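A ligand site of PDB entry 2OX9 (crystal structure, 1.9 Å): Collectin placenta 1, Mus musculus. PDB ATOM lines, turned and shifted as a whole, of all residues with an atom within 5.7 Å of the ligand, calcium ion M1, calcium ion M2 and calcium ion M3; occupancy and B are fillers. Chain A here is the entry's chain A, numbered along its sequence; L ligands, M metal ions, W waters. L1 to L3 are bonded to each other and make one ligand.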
ATOM      1  N   ASP A  68     -11.305 -11.548 -10.418  1.00  0.00           N
ATOM      2  CA  ASP A  68     -11.823 -10.190 -10.543  1.00  0.00           C
ATOM      3  C   ASP A  68     -12.720 -10.147 -11.784  1.00  0.00           C
ATOM      4  O   ASP A  68     -12.753  -9.155 -12.514  1.00  0.00           O
ATOM      5  CB  ASP A  68     -10.671  -9.158 -10.624  1.00  0.00           C
ATOM      6  CG  ASP A  68      -9.958  -9.177 -11.967  1.00  0.00           C
ATOM      7  OD1 ASP A  68      -9.968 -10.208 -12.645  1.00  0.00           O
ATOM      8  OD2 ASP A  68      -9.369  -8.132 -12.335  1.00  0.00           O
ATOM      9  N   SER A  69     -13.437 -11.245 -11.998  1.00  0.00           N
ATOM     10  CA  SER A  69     -14.362 -11.386 -13.123  1.00  0.00           C
ATOM     11  C   SER A  69     -15.618 -10.547 -12.923  1.00  0.00           C
ATOM     12  O   SER A  69     -16.160 -10.011 -13.883  1.00  0.00           O
ATOM     13  CB  SER A  69     -14.775 -12.845 -13.300  1.00  0.00           C
ATOM     14  OG  SER A  69     -13.673 -13.669 -13.634  1.00  0.00           O
ATOM     15  N   GLU A  72     -13.592  -5.911 -12.967  1.00  0.00           N
ATOM     16  CA  GLU A  72     -12.162  -5.775 -13.208  1.00  0.00           C
ATOM     17  C   GLU A  72     -11.455  -4.984 -12.099  1.00  0.00           C
ATOM     18  O   GLU A  72     -11.926  -3.921 -11.686  1.00  0.00           O
ATOM     19  CB  GLU A  72     -11.927  -5.122 -14.571  1.00  0.00           C
ATOM     20  CG  GLU A  72     -10.477  -5.027 -15.021  1.00  0.00           C
ATOM     21  CD  GLU A  72      -9.785  -6.382 -15.069  1.00  0.00           C
ATOM     22  OE1 GLU A  72     -10.442  -7.362 -15.476  1.00  0.00           O
ATOM     23  OE2 GLU A  72      -8.599  -6.464 -14.719  1.00  0.00           O
ATOM     24  N   SER A  73     -10.334  -5.522 -11.628  1.00  0.00           N
ATOM     25  CA  SER A  73      -9.512  -4.921 -10.579  1.00  0.00           C
ATOM     26  C   SER A  73     -10.031  -5.054  -9.162  1.00  0.00           C
ATOM     27  O   SER A  73      -9.366  -4.657  -8.211  1.00  0.00           O
ATOM     28  CB  SER A  73      -9.230  -3.445 -10.882  1.00  0.00           C
ATOM     29  OG  SER A  73      -8.318  -3.328 -11.961  1.00  0.00           O
ATOM     30  N   TRP A  75     -10.554  -7.657  -6.804  1.00  0.00           N
ATOM     31  CA  TRP A  75     -10.247  -9.042  -6.481  1.00  0.00           C
ATOM     32  C   TRP A  75     -10.900  -9.556  -5.205  1.00  0.00           C
ATOM     33  O   TRP A  75     -10.804  -8.920  -4.164  1.00  0.00           O
ATOM     34  CB  TRP A  75      -8.727  -9.240  -6.413  1.00  0.00           C
ATOM     35  CG  TRP A  75      -8.055  -9.094  -7.742  1.00  0.00           C
ATOM     36  CD1 TRP A  75      -7.617  -7.931  -8.314  1.00  0.00           C
ATOM     37  CD2 TRP A  75      -7.789 -10.133  -8.687  1.00  0.00           C
ATOM     38  NE1 TRP A  75      -7.091  -8.198  -9.556  1.00  0.00           N
ATOM     39  CE2 TRP A  75      -7.185  -9.540  -9.810  1.00  0.00           C
ATOM     40  CE3 TRP A  75      -8.011 -11.524  -8.689  1.00  0.00           C
ATOM     41  CZ2 TRP A  75      -6.786 -10.277 -10.929  1.00  0.00           C
ATOM     42  CZ3 TRP A  75      -7.613 -12.253  -9.802  1.00  0.00           C
ATOM     43  CH2 TRP A  75      -7.017 -11.630 -10.913  1.00  0.00           C
ATOM     44  N   LYS A  89       3.149 -10.469  -7.516  1.00  0.00           N
ATOM     45  CA  LYS A  89       4.512 -10.217  -7.916  1.00  0.00           C
ATOM     46  C   LYS A  89       4.465  -8.753  -8.363  1.00  0.00           C
ATOM     47  O   LYS A  89       3.413  -8.272  -8.787  1.00  0.00           O
ATOM     48  CB  LYS A  89       4.888 -11.118  -9.106  1.00  0.00           C
ATOM     49  CG  LYS A  89       6.247 -10.798  -9.731  1.00  0.00           C
ATOM     50  CD  LYS A  89       6.507 -11.670 -10.937  1.00  0.00           C
ATOM     51  CE  LYS A  89       7.826 -11.318 -11.612  1.00  0.00           C
ATOM     52  NZ  LYS A  89       8.032 -12.140 -12.827  1.00  0.00           N
ATOM     53  N   ALA A  90       5.583  -8.037  -8.257  1.00  0.00           N
ATOM     54  CA  ALA A  90       5.612  -6.630  -8.642  1.00  0.00           C
ATOM     55  C   ALA A  90       5.215  -6.481 -10.117  1.00  0.00           C
ATOM     56  O   ALA A  90       5.750  -7.173 -10.974  1.00  0.00           O
ATOM     57  CB  ALA A  90       6.999  -6.051  -8.404  1.00  0.00           C
ATOM     58  N   GLN A  92       2.226  -7.066 -11.212  1.00  0.00           N
ATOM     59  CA  GLN A  92       0.987  -7.818 -11.351  1.00  0.00           C
ATOM     60  C   GLN A  92      -0.018  -7.296 -10.324  1.00  0.00           C
ATOM     61  O   GLN A  92       0.367  -6.785  -9.285  1.00  0.00           O
ATOM     62  CB  GLN A  92       1.239  -9.305 -11.107  1.00  0.00           C
ATOM     63  CG  GLN A  92       2.176  -9.924 -12.100  1.00  0.00           C
ATOM     64  CD  GLN A  92       1.776  -9.593 -13.523  1.00  0.00           C
ATOM     65  OE1 GLN A  92       0.672  -9.906 -13.959  1.00  0.00           O
ATOM     66  NE2 GLN A  92       2.683  -8.945 -14.250  1.00  0.00           N
ATOM     67  N   PRO A  93      -1.329  -7.415 -10.612  1.00  0.00           N
ATOM     68  CA  PRO A  93      -1.957  -7.993 -11.811  1.00  0.00           C
ATOM     69  C   PRO A  93      -1.887  -7.023 -12.984  1.00  0.00           C
ATOM     70  O   PRO A  93      -2.046  -5.821 -12.807  1.00  0.00           O
ATOM     71  CB  PRO A  93      -3.391  -8.268 -11.354  1.00  0.00           C
ATOM     72  CG  PRO A  93      -3.630  -7.187 -10.337  1.00  0.00           C
ATOM     73  CD  PRO A  93      -2.348  -7.148  -9.570  1.00  0.00           C
ATOM     74  N   ASP A  94      -1.632  -7.536 -14.184  1.00  0.00           N
ATOM     75  CA  ASP A  94      -1.514  -6.657 -15.346  1.00  0.00           C
ATOM     76  C   ASP A  94      -2.652  -6.763 -16.356  1.00  0.00           C
ATOM     77  O   ASP A  94      -2.687  -6.004 -17.321  1.00  0.00           O
ATOM     78  CB  ASP A  94      -0.168  -6.888 -16.031  1.00  0.00           C
ATOM     79  CG  ASP A  94      -0.005  -8.306 -16.550  1.00  0.00           C
ATOM     80  OD1 ASP A  94      -0.882  -9.145 -16.271  1.00  0.00           O
ATOM     81  OD2 ASP A  94       1.001  -8.577 -17.243  1.00  0.00           O
ATOM     82  N   ASN A  95      -3.565  -7.706 -16.139  1.00  0.00           N
ATOM     83  CA  ASN A  95      -4.712  -7.920 -17.029  1.00  0.00           C
ATOM     84  C   ASN A  95      -4.262  -7.972 -18.492  1.00  0.00           C
ATOM     85  O   ASN A  95      -4.889  -7.385 -19.373  1.00  0.00           O
ATOM     86  CB  ASN A  95      -5.726  -6.778 -16.826  1.00  0.00           C
ATOM     87  CG  ASN A  95      -7.156  -7.204 -17.130  1.00  0.00           C
ATOM     88  OD1 ASN A  95      -7.616  -8.263 -16.674  1.00  0.00           O
ATOM     89  ND2 ASN A  95      -7.868  -6.378 -17.885  1.00  0.00           N
ATOM     90  N   TRP A  96      -3.188  -8.696 -18.743  1.00  0.00           N
ATOM     91  CA  TRP A  96      -2.613  -8.838 -20.079  1.00  0.00           C
ATOM     92  C   TRP A  96      -3.657  -9.258 -21.115  1.00  0.00           C
ATOM     93  O   TRP A  96      -4.456 -10.159 -20.873  1.00  0.00           O
ATOM     94  CB  TRP A  96      -1.482  -9.863 -20.040  1.00  0.00           C
ATOM     95  CG  TRP A  96      -0.477  -9.738 -21.129  1.00  0.00           C
ATOM     96  CD1 TRP A  96      -0.236 -10.632 -22.129  1.00  0.00           C
ATOM     97  CD2 TRP A  96       0.468  -8.668 -21.308  1.00  0.00           C
ATOM     98  NE1 TRP A  96       0.806 -10.184 -22.920  1.00  0.00           N
ATOM     99  CE2 TRP A  96       1.248  -8.986 -22.438  1.00  0.00           C
ATOM    100  CE3 TRP A  96       0.724  -7.470 -20.627  1.00  0.00           C
ATOM    101  CZ2 TRP A  96       2.278  -8.155 -22.892  1.00  0.00           C
ATOM    102  CZ3 TRP A  96       1.743  -6.638 -21.081  1.00  0.00           C
ATOM    103  CH2 TRP A  96       2.507  -6.997 -22.211  1.00  0.00           C
ATOM    104  N   PRO A 102     -11.386 -10.319 -22.267  1.00  0.00           N
ATOM    105  CA  PRO A 102     -11.610  -9.993 -20.859  1.00  0.00           C
ATOM    106  C   PRO A 102     -10.343  -9.841 -20.022  1.00  0.00           C
ATOM    107  O   PRO A 102     -10.404  -9.491 -18.839  1.00  0.00           O
ATOM    108  CB  PRO A 102     -12.483 -11.158 -20.380  1.00  0.00           C
ATOM    109  CG  PRO A 102     -11.933 -12.293 -21.179  1.00  0.00           C
ATOM    110  CD  PRO A 102     -11.775 -11.709 -22.567  1.00  0.00           C
ATOM    111  N   GLY A 103      -9.194 -10.121 -20.649  1.00  0.00           N
ATOM    112  CA  GLY A 103      -7.934 -10.003 -19.953  1.00  0.00           C
ATOM    113  C   GLY A 103      -7.610 -11.199 -19.077  1.00  0.00           C
ATOM    114  O   GLY A 103      -7.824 -12.346 -19.471  1.00  0.00           O
ATOM    115  N   GLU A 104      -7.104 -10.926 -17.880  1.00  0.00           N
ATOM    116  CA  GLU A 104      -6.741 -11.974 -16.915  1.00  0.00           C
ATOM    117  C   GLU A 104      -7.545 -11.718 -15.655  1.00  0.00           C
ATOM    118  O   GLU A 104      -7.339 -10.720 -14.960  1.00  0.00           O
ATOM    119  CB  GLU A 104      -5.236 -11.916 -16.623  1.00  0.00           C
ATOM    120  CG  GLU A 104      -4.377 -12.072 -17.890  1.00  0.00           C
ATOM    121  CD  GLU A 104      -2.893 -12.183 -17.603  1.00  0.00           C
ATOM    122  OE1 GLU A 104      -2.303 -11.217 -17.075  1.00  0.00           O
ATOM    123  OE2 GLU A 104      -2.303 -13.243 -17.903  1.00  0.00           O
ATOM    124  N   ASP A 105      -8.448 -12.636 -15.331  1.00  0.00           N
ATOM    125  CA  ASP A 105      -9.300 -12.458 -14.179  1.00  0.00           C
ATOM    126  C   ASP A 105      -9.242 -13.596 -13.152  1.00  0.00           C
ATOM    127  O   ASP A 105     -10.105 -13.686 -12.269  1.00  0.00           O
ATOM    128  CB  ASP A 105     -10.753 -12.281 -14.645  1.00  0.00           C
ATOM    129  CG  ASP A 105     -10.916 -11.126 -15.628  1.00  0.00           C
ATOM    130  OD1 ASP A 105      -9.947 -10.354 -15.821  1.00  0.00           O
ATOM    131  OD2 ASP A 105     -12.017 -11.003 -16.206  1.00  0.00           O
ATOM    132  N   ILE A 110       2.898 -18.465  -8.858  1.00  0.00           N
ATOM    133  CA  ILE A 110       3.987 -18.715  -9.786  1.00  0.00           C
ATOM    134  C   ILE A 110       5.304 -18.866  -9.017  1.00  0.00           C
ATOM    135  O   ILE A 110       5.302 -19.348  -7.881  1.00  0.00           O
ATOM    136  CB  ILE A 110       4.104 -17.581 -10.842  1.00  0.00           C
ATOM    137  CG1 ILE A 110       4.124 -16.229 -10.148  1.00  0.00           C
ATOM    138  CG2 ILE A 110       2.943 -17.683 -11.827  1.00  0.00           C
ATOM    139  CD1 ILE A 110       4.344 -15.068 -11.102  1.00  0.00           C
ATOM    140  N   ASN A 116       0.030 -14.122  -9.652  1.00  0.00           N
ATOM    141  CA  ASN A 116      -0.058 -13.573 -10.980  1.00  0.00           C
ATOM    142  C   ASN A 116      -1.467 -13.805 -11.500  1.00  0.00           C
ATOM    143  O   ASN A 116      -2.108 -14.786 -11.142  1.00  0.00           O
ATOM    144  CB  ASN A 116       0.935 -14.246 -11.914  1.00  0.00           C
ATOM    145  CG  ASN A 116       0.682 -13.901 -13.356  1.00  0.00           C
ATOM    146  OD1 ASN A 116       0.597 -12.720 -13.711  1.00  0.00           O
ATOM    147  ND2 ASN A 116       0.562 -14.918 -14.197  1.00  0.00           N
ATOM    148  N   ASP A 117      -1.955 -12.898 -12.335  1.00  0.00           N
ATOM    149  CA  ASP A 117      -3.277 -13.059 -12.906  1.00  0.00           C
ATOM    150  C   ASP A 117      -3.124 -13.723 -14.266  1.00  0.00           C
ATOM    151  O   ASP A 117      -2.245 -13.352 -15.057  1.00  0.00           O
ATOM    152  CB  ASP A 117      -3.987 -11.681 -13.019  1.00  0.00           C
ATOM    153  CG  ASP A 117      -3.167 -10.643 -13.774  1.00  0.00           C
ATOM    154  OD1 ASP A 117      -1.918 -10.721 -13.774  1.00  0.00           O
ATOM    155  OD2 ASP A 117      -3.776  -9.715 -14.360  1.00  0.00           O
ATOM    156  N   PHE A 118      -3.938 -14.745 -14.517  1.00  0.00           N
ATOM    157  CA  PHE A 118      -3.898 -15.482 -15.778  1.00  0.00           C
ATOM    158  C   PHE A 118      -5.266 -15.390 -16.449  1.00  0.00           C
ATOM    159  O   PHE A 118      -6.264 -15.038 -15.817  1.00  0.00           O
ATOM    160  CB  PHE A 118      -3.653 -16.985 -15.576  1.00  0.00           C
ATOM    161  CG  PHE A 118      -2.387 -17.323 -14.837  1.00  0.00           C
ATOM    162  CD1 PHE A 118      -2.352 -17.291 -13.451  1.00  0.00           C
ATOM    163  CD2 PHE A 118      -1.274 -17.787 -15.527  1.00  0.00           C
ATOM    164  CE1 PHE A 118      -1.222 -17.706 -12.759  1.00  0.00           C
ATOM    165  CE2 PHE A 118      -0.135 -18.211 -14.840  1.00  0.00           C
ATOM    166  CZ  PHE A 118      -0.110 -18.170 -13.449  1.00  0.00           C
HETATM  167  C1  LIG L   1       7.250 -12.734 -16.475  1.00  0.00           C
HETATM  168  C2  LIG L   1       7.673 -11.254 -16.441  1.00  0.00           C
HETATM  169  C3  LIG L   1       6.438 -10.359 -16.513  1.00  0.00           C
HETATM  170  C4  LIG L   1       5.459 -10.730 -15.405  1.00  0.00           C
HETATM  171  C5  LIG L   1       5.094 -12.214 -15.510  1.00  0.00           C
HETATM  172  C6  LIG L   1       4.173 -12.663 -14.377  1.00  0.00           C
HETATM  173  O1  LIG L   1       8.528 -10.973 -17.537  1.00  0.00           O
HETATM  174  O2  LIG L   1       6.825  -8.999 -16.390  1.00  0.00           O
HETATM  175  O3  LIG L   1       6.048 -10.465 -14.141  1.00  0.00           O
HETATM  176  O4  LIG L   1       6.292 -13.026 -15.455  1.00  0.00           O
HETATM  177  C1  LG2 L   2       7.761 -16.328 -19.384  1.00  0.00           C
HETATM  178  C2  LG2 L   2       7.867 -14.853 -19.009  1.00  0.00           C
HETATM  179  C3  LG2 L   2       6.749 -14.476 -18.042  1.00  0.00           C
HETATM  180  C4  LG2 L   2       5.397 -14.834 -18.662  1.00  0.00           C
HETATM  181  C5  LG2 L   2       5.385 -16.309 -19.055  1.00  0.00           C
HETATM  182  C6  LG2 L   2       4.103 -16.696 -19.779  1.00  0.00           C
HETATM  183  C7  LG2 L   2       9.863 -13.523 -18.782  1.00  0.00           C
HETATM  184  C8  LG2 L   2      11.347 -13.533 -18.474  1.00  0.00           C
HETATM  185  N1  LG2 L   2       9.167 -14.596 -18.410  1.00  0.00           N
HETATM  186  O1  LG2 L   2       8.732 -16.634 -20.322  1.00  0.00           O
HETATM  187  O2  LG2 L   2       6.796 -13.068 -17.755  1.00  0.00           O
HETATM  188  O3  LG2 L   2       4.340 -14.566 -17.725  1.00  0.00           O
HETATM  189  O4  LG2 L   2       6.478 -16.587 -19.966  1.00  0.00           O
HETATM  190  O5  LG2 L   2       3.884 -15.869 -20.905  1.00  0.00           O
HETATM  191  O6  LG2 L   2       9.349 -12.543 -19.339  1.00  0.00           O
HETATM  192  C1  LG3 L   3       3.242 -13.875 -18.217  1.00  0.00           C
HETATM  193  C2  LG3 L   3       2.073 -14.040 -17.244  1.00  0.00           C
HETATM  194  C3  LG3 L   3       0.879 -13.191 -17.700  1.00  0.00           C
HETATM  195  C4  LG3 L   3       1.304 -11.746 -17.956  1.00  0.00           C
HETATM  196  C5  LG3 L   3       2.524 -11.693 -18.881  1.00  0.00           C
HETATM  197  C6  LG3 L   3       3.066 -10.282 -19.057  1.00  0.00           C
HETATM  198  O1  LG3 L   3       1.695 -15.400 -17.188  1.00  0.00           O
HETATM  199  O2  LG3 L   3      -0.115 -13.228 -16.694  1.00  0.00           O
HETATM  200  O3  LG3 L   3       1.609 -11.115 -16.720  1.00  0.00           O
HETATM  201  O4  LG3 L   3       3.601 -12.494 -18.341  1.00  0.00           O
HETATM  202  O5  LG3 L   3       3.964 -10.207 -20.148  1.00  0.00           O
HETATM  203 CA    CA M   1      -8.593  -8.848 -14.504  1.00  0.00          CA
HETATM  204 CA    CA M   2      -0.672 -11.436 -15.310  1.00  0.00          CA
HETATM  205 CA    CA M   3     -11.557  -8.825 -16.875  1.00  0.00          CA
HETATM  206  O   HOH W   1     -11.355  -6.739 -18.260  1.00  0.00           O
HETATM  207  O   HOH W   2       0.078 -16.429 -18.837  1.00  0.00           O
HETATM  208  O   HOH W   3     -12.946  -8.299 -15.365  1.00  0.00           O
HETATM  209  O   HOH W   4      -6.053  -8.256 -14.125  1.00  0.00           O
HETATM  210  O   HOH W   5       7.051  -7.007 -18.480  1.00  0.00           O
HETATM  211  O   HOH W   6       5.336  -8.141 -13.736  1.00  0.00           O
HETATM  212  O   HOH W   7       3.267 -16.612 -15.587  1.00  0.00           O
HETATM  213  O   HOH W   8       6.060 -16.388 -14.849  1.00  0.00           O
HETATM  214  O   HOH W   9       8.594  -8.197 -14.088  1.00  0.00           O
HETATM  215  O   HOH W  10       5.565  -6.065 -15.260  1.00  0.00           O
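Water W4 bridges the side-chain carboxylate of Asp 117 (2.7 Å) and the backbone NH of Asn 95 (3.2 Å).
Water W6 lies within hydrogen-bond range of an oxygen (O3) of LIG L1 (2.5 Å), the side-chain amide nitrogen of Gln 92 (2.8 Å) and the backbone carbonyl oxygen of Ala 90 (3.0 Å).
Water W7 bridges O1 of LG3 L3 (2.6 Å) and ND2 of Asn 116 (3.5 Å).
The nearest printed residue that does not touch calcium ion M1 is Trp 75 (4.3 Å).
CE2 of Trp 96 touches O5 of LG3 L3 (3.8 Å).
Hydrophobic or aromatic side chains within 4 Å of the ligand: Trp 96.
Five residues have an atom within 4 Å of calcium ion M2: Gln 92, Asp 94, Glu 104, Asn 116 and Asp 117.
An oxygen (O3) of LIG L1 is in hydrogen-bond range of the side-chain amino group (NZ) of Lys 89, at 2.9 Å.
Along chain A the residues within 4 Å of calcium ion M3 span positions 72 to 105.
The nearest printed residue that does not touch calcium ion M3 is Asp 68 (4.5 Å).
Calcium ion M3 is bound by water W3 (2.1 Å), OE1 of Glu 72 (2.3 Å), OD2 of Asp 105 (2.3 Å), O of Pro 102 (2.4 Å), OD1 of Asp 105 (2.5 Å) and water W1 (2.5 Å).
Calcium ion M2 is bound by the side-chain carboxylate (OD1) of Asp 117 (2.1 Å), an oxygen (O2) of LG3 L3 (2.3 Å), the side-chain amide oxygen (OD1) of Asn 116 (2.4 Å), the side-chain carboxylate (OE1) of Glu 104 (2.4 Å), the side-chain amide oxygen (OE1) of Gln 92 (2.4 Å), the backbone carbonyl oxygen (O) of Asp 117 (2.5 Å), the side-chain carboxylate (OD1) of Asp 94 (2.5 Å) and an oxygen (O3) of LG3 L3 (2.7 Å).
Calcium ion M1 is bound by O of Glu 104 (2.3 Å), OE2 of Glu 72 (2.4 Å), OD2 of Asp 68 (2.4 Å), OD1 of Asp 105 (2.4 Å), OD1 of Asn 95 (2.5 Å), OE1 of Glu 72 (2.6 Å), water W4 (2.6 Å) and OD1 of Asp 68 (2.7 Å).
Calcium ion M1 has eight donor atoms within binding distance.
The side-chain carboxylate (OD2) of Asp 117 lies within hydrogen-bond range of the backbone NH (N) of Asn 95, at 2.7 Å.
The side-chain carboxylate (OE1) of Glu 104 lies close to the backbone NH (N) of Trp 96 (3.1 Å).
N of Asp 105 is in hydrogen-bond range of O of Phe 118 (3.3 Å).
The backbone NH (N) of Ser 73 lies close to the side-chain carboxylate (OD2) of Asp 68, at 2.9 Å.
The side-chain carboxylate (OD1) of Asp 94 lies close to the backbone NH (N) of Trp 96.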
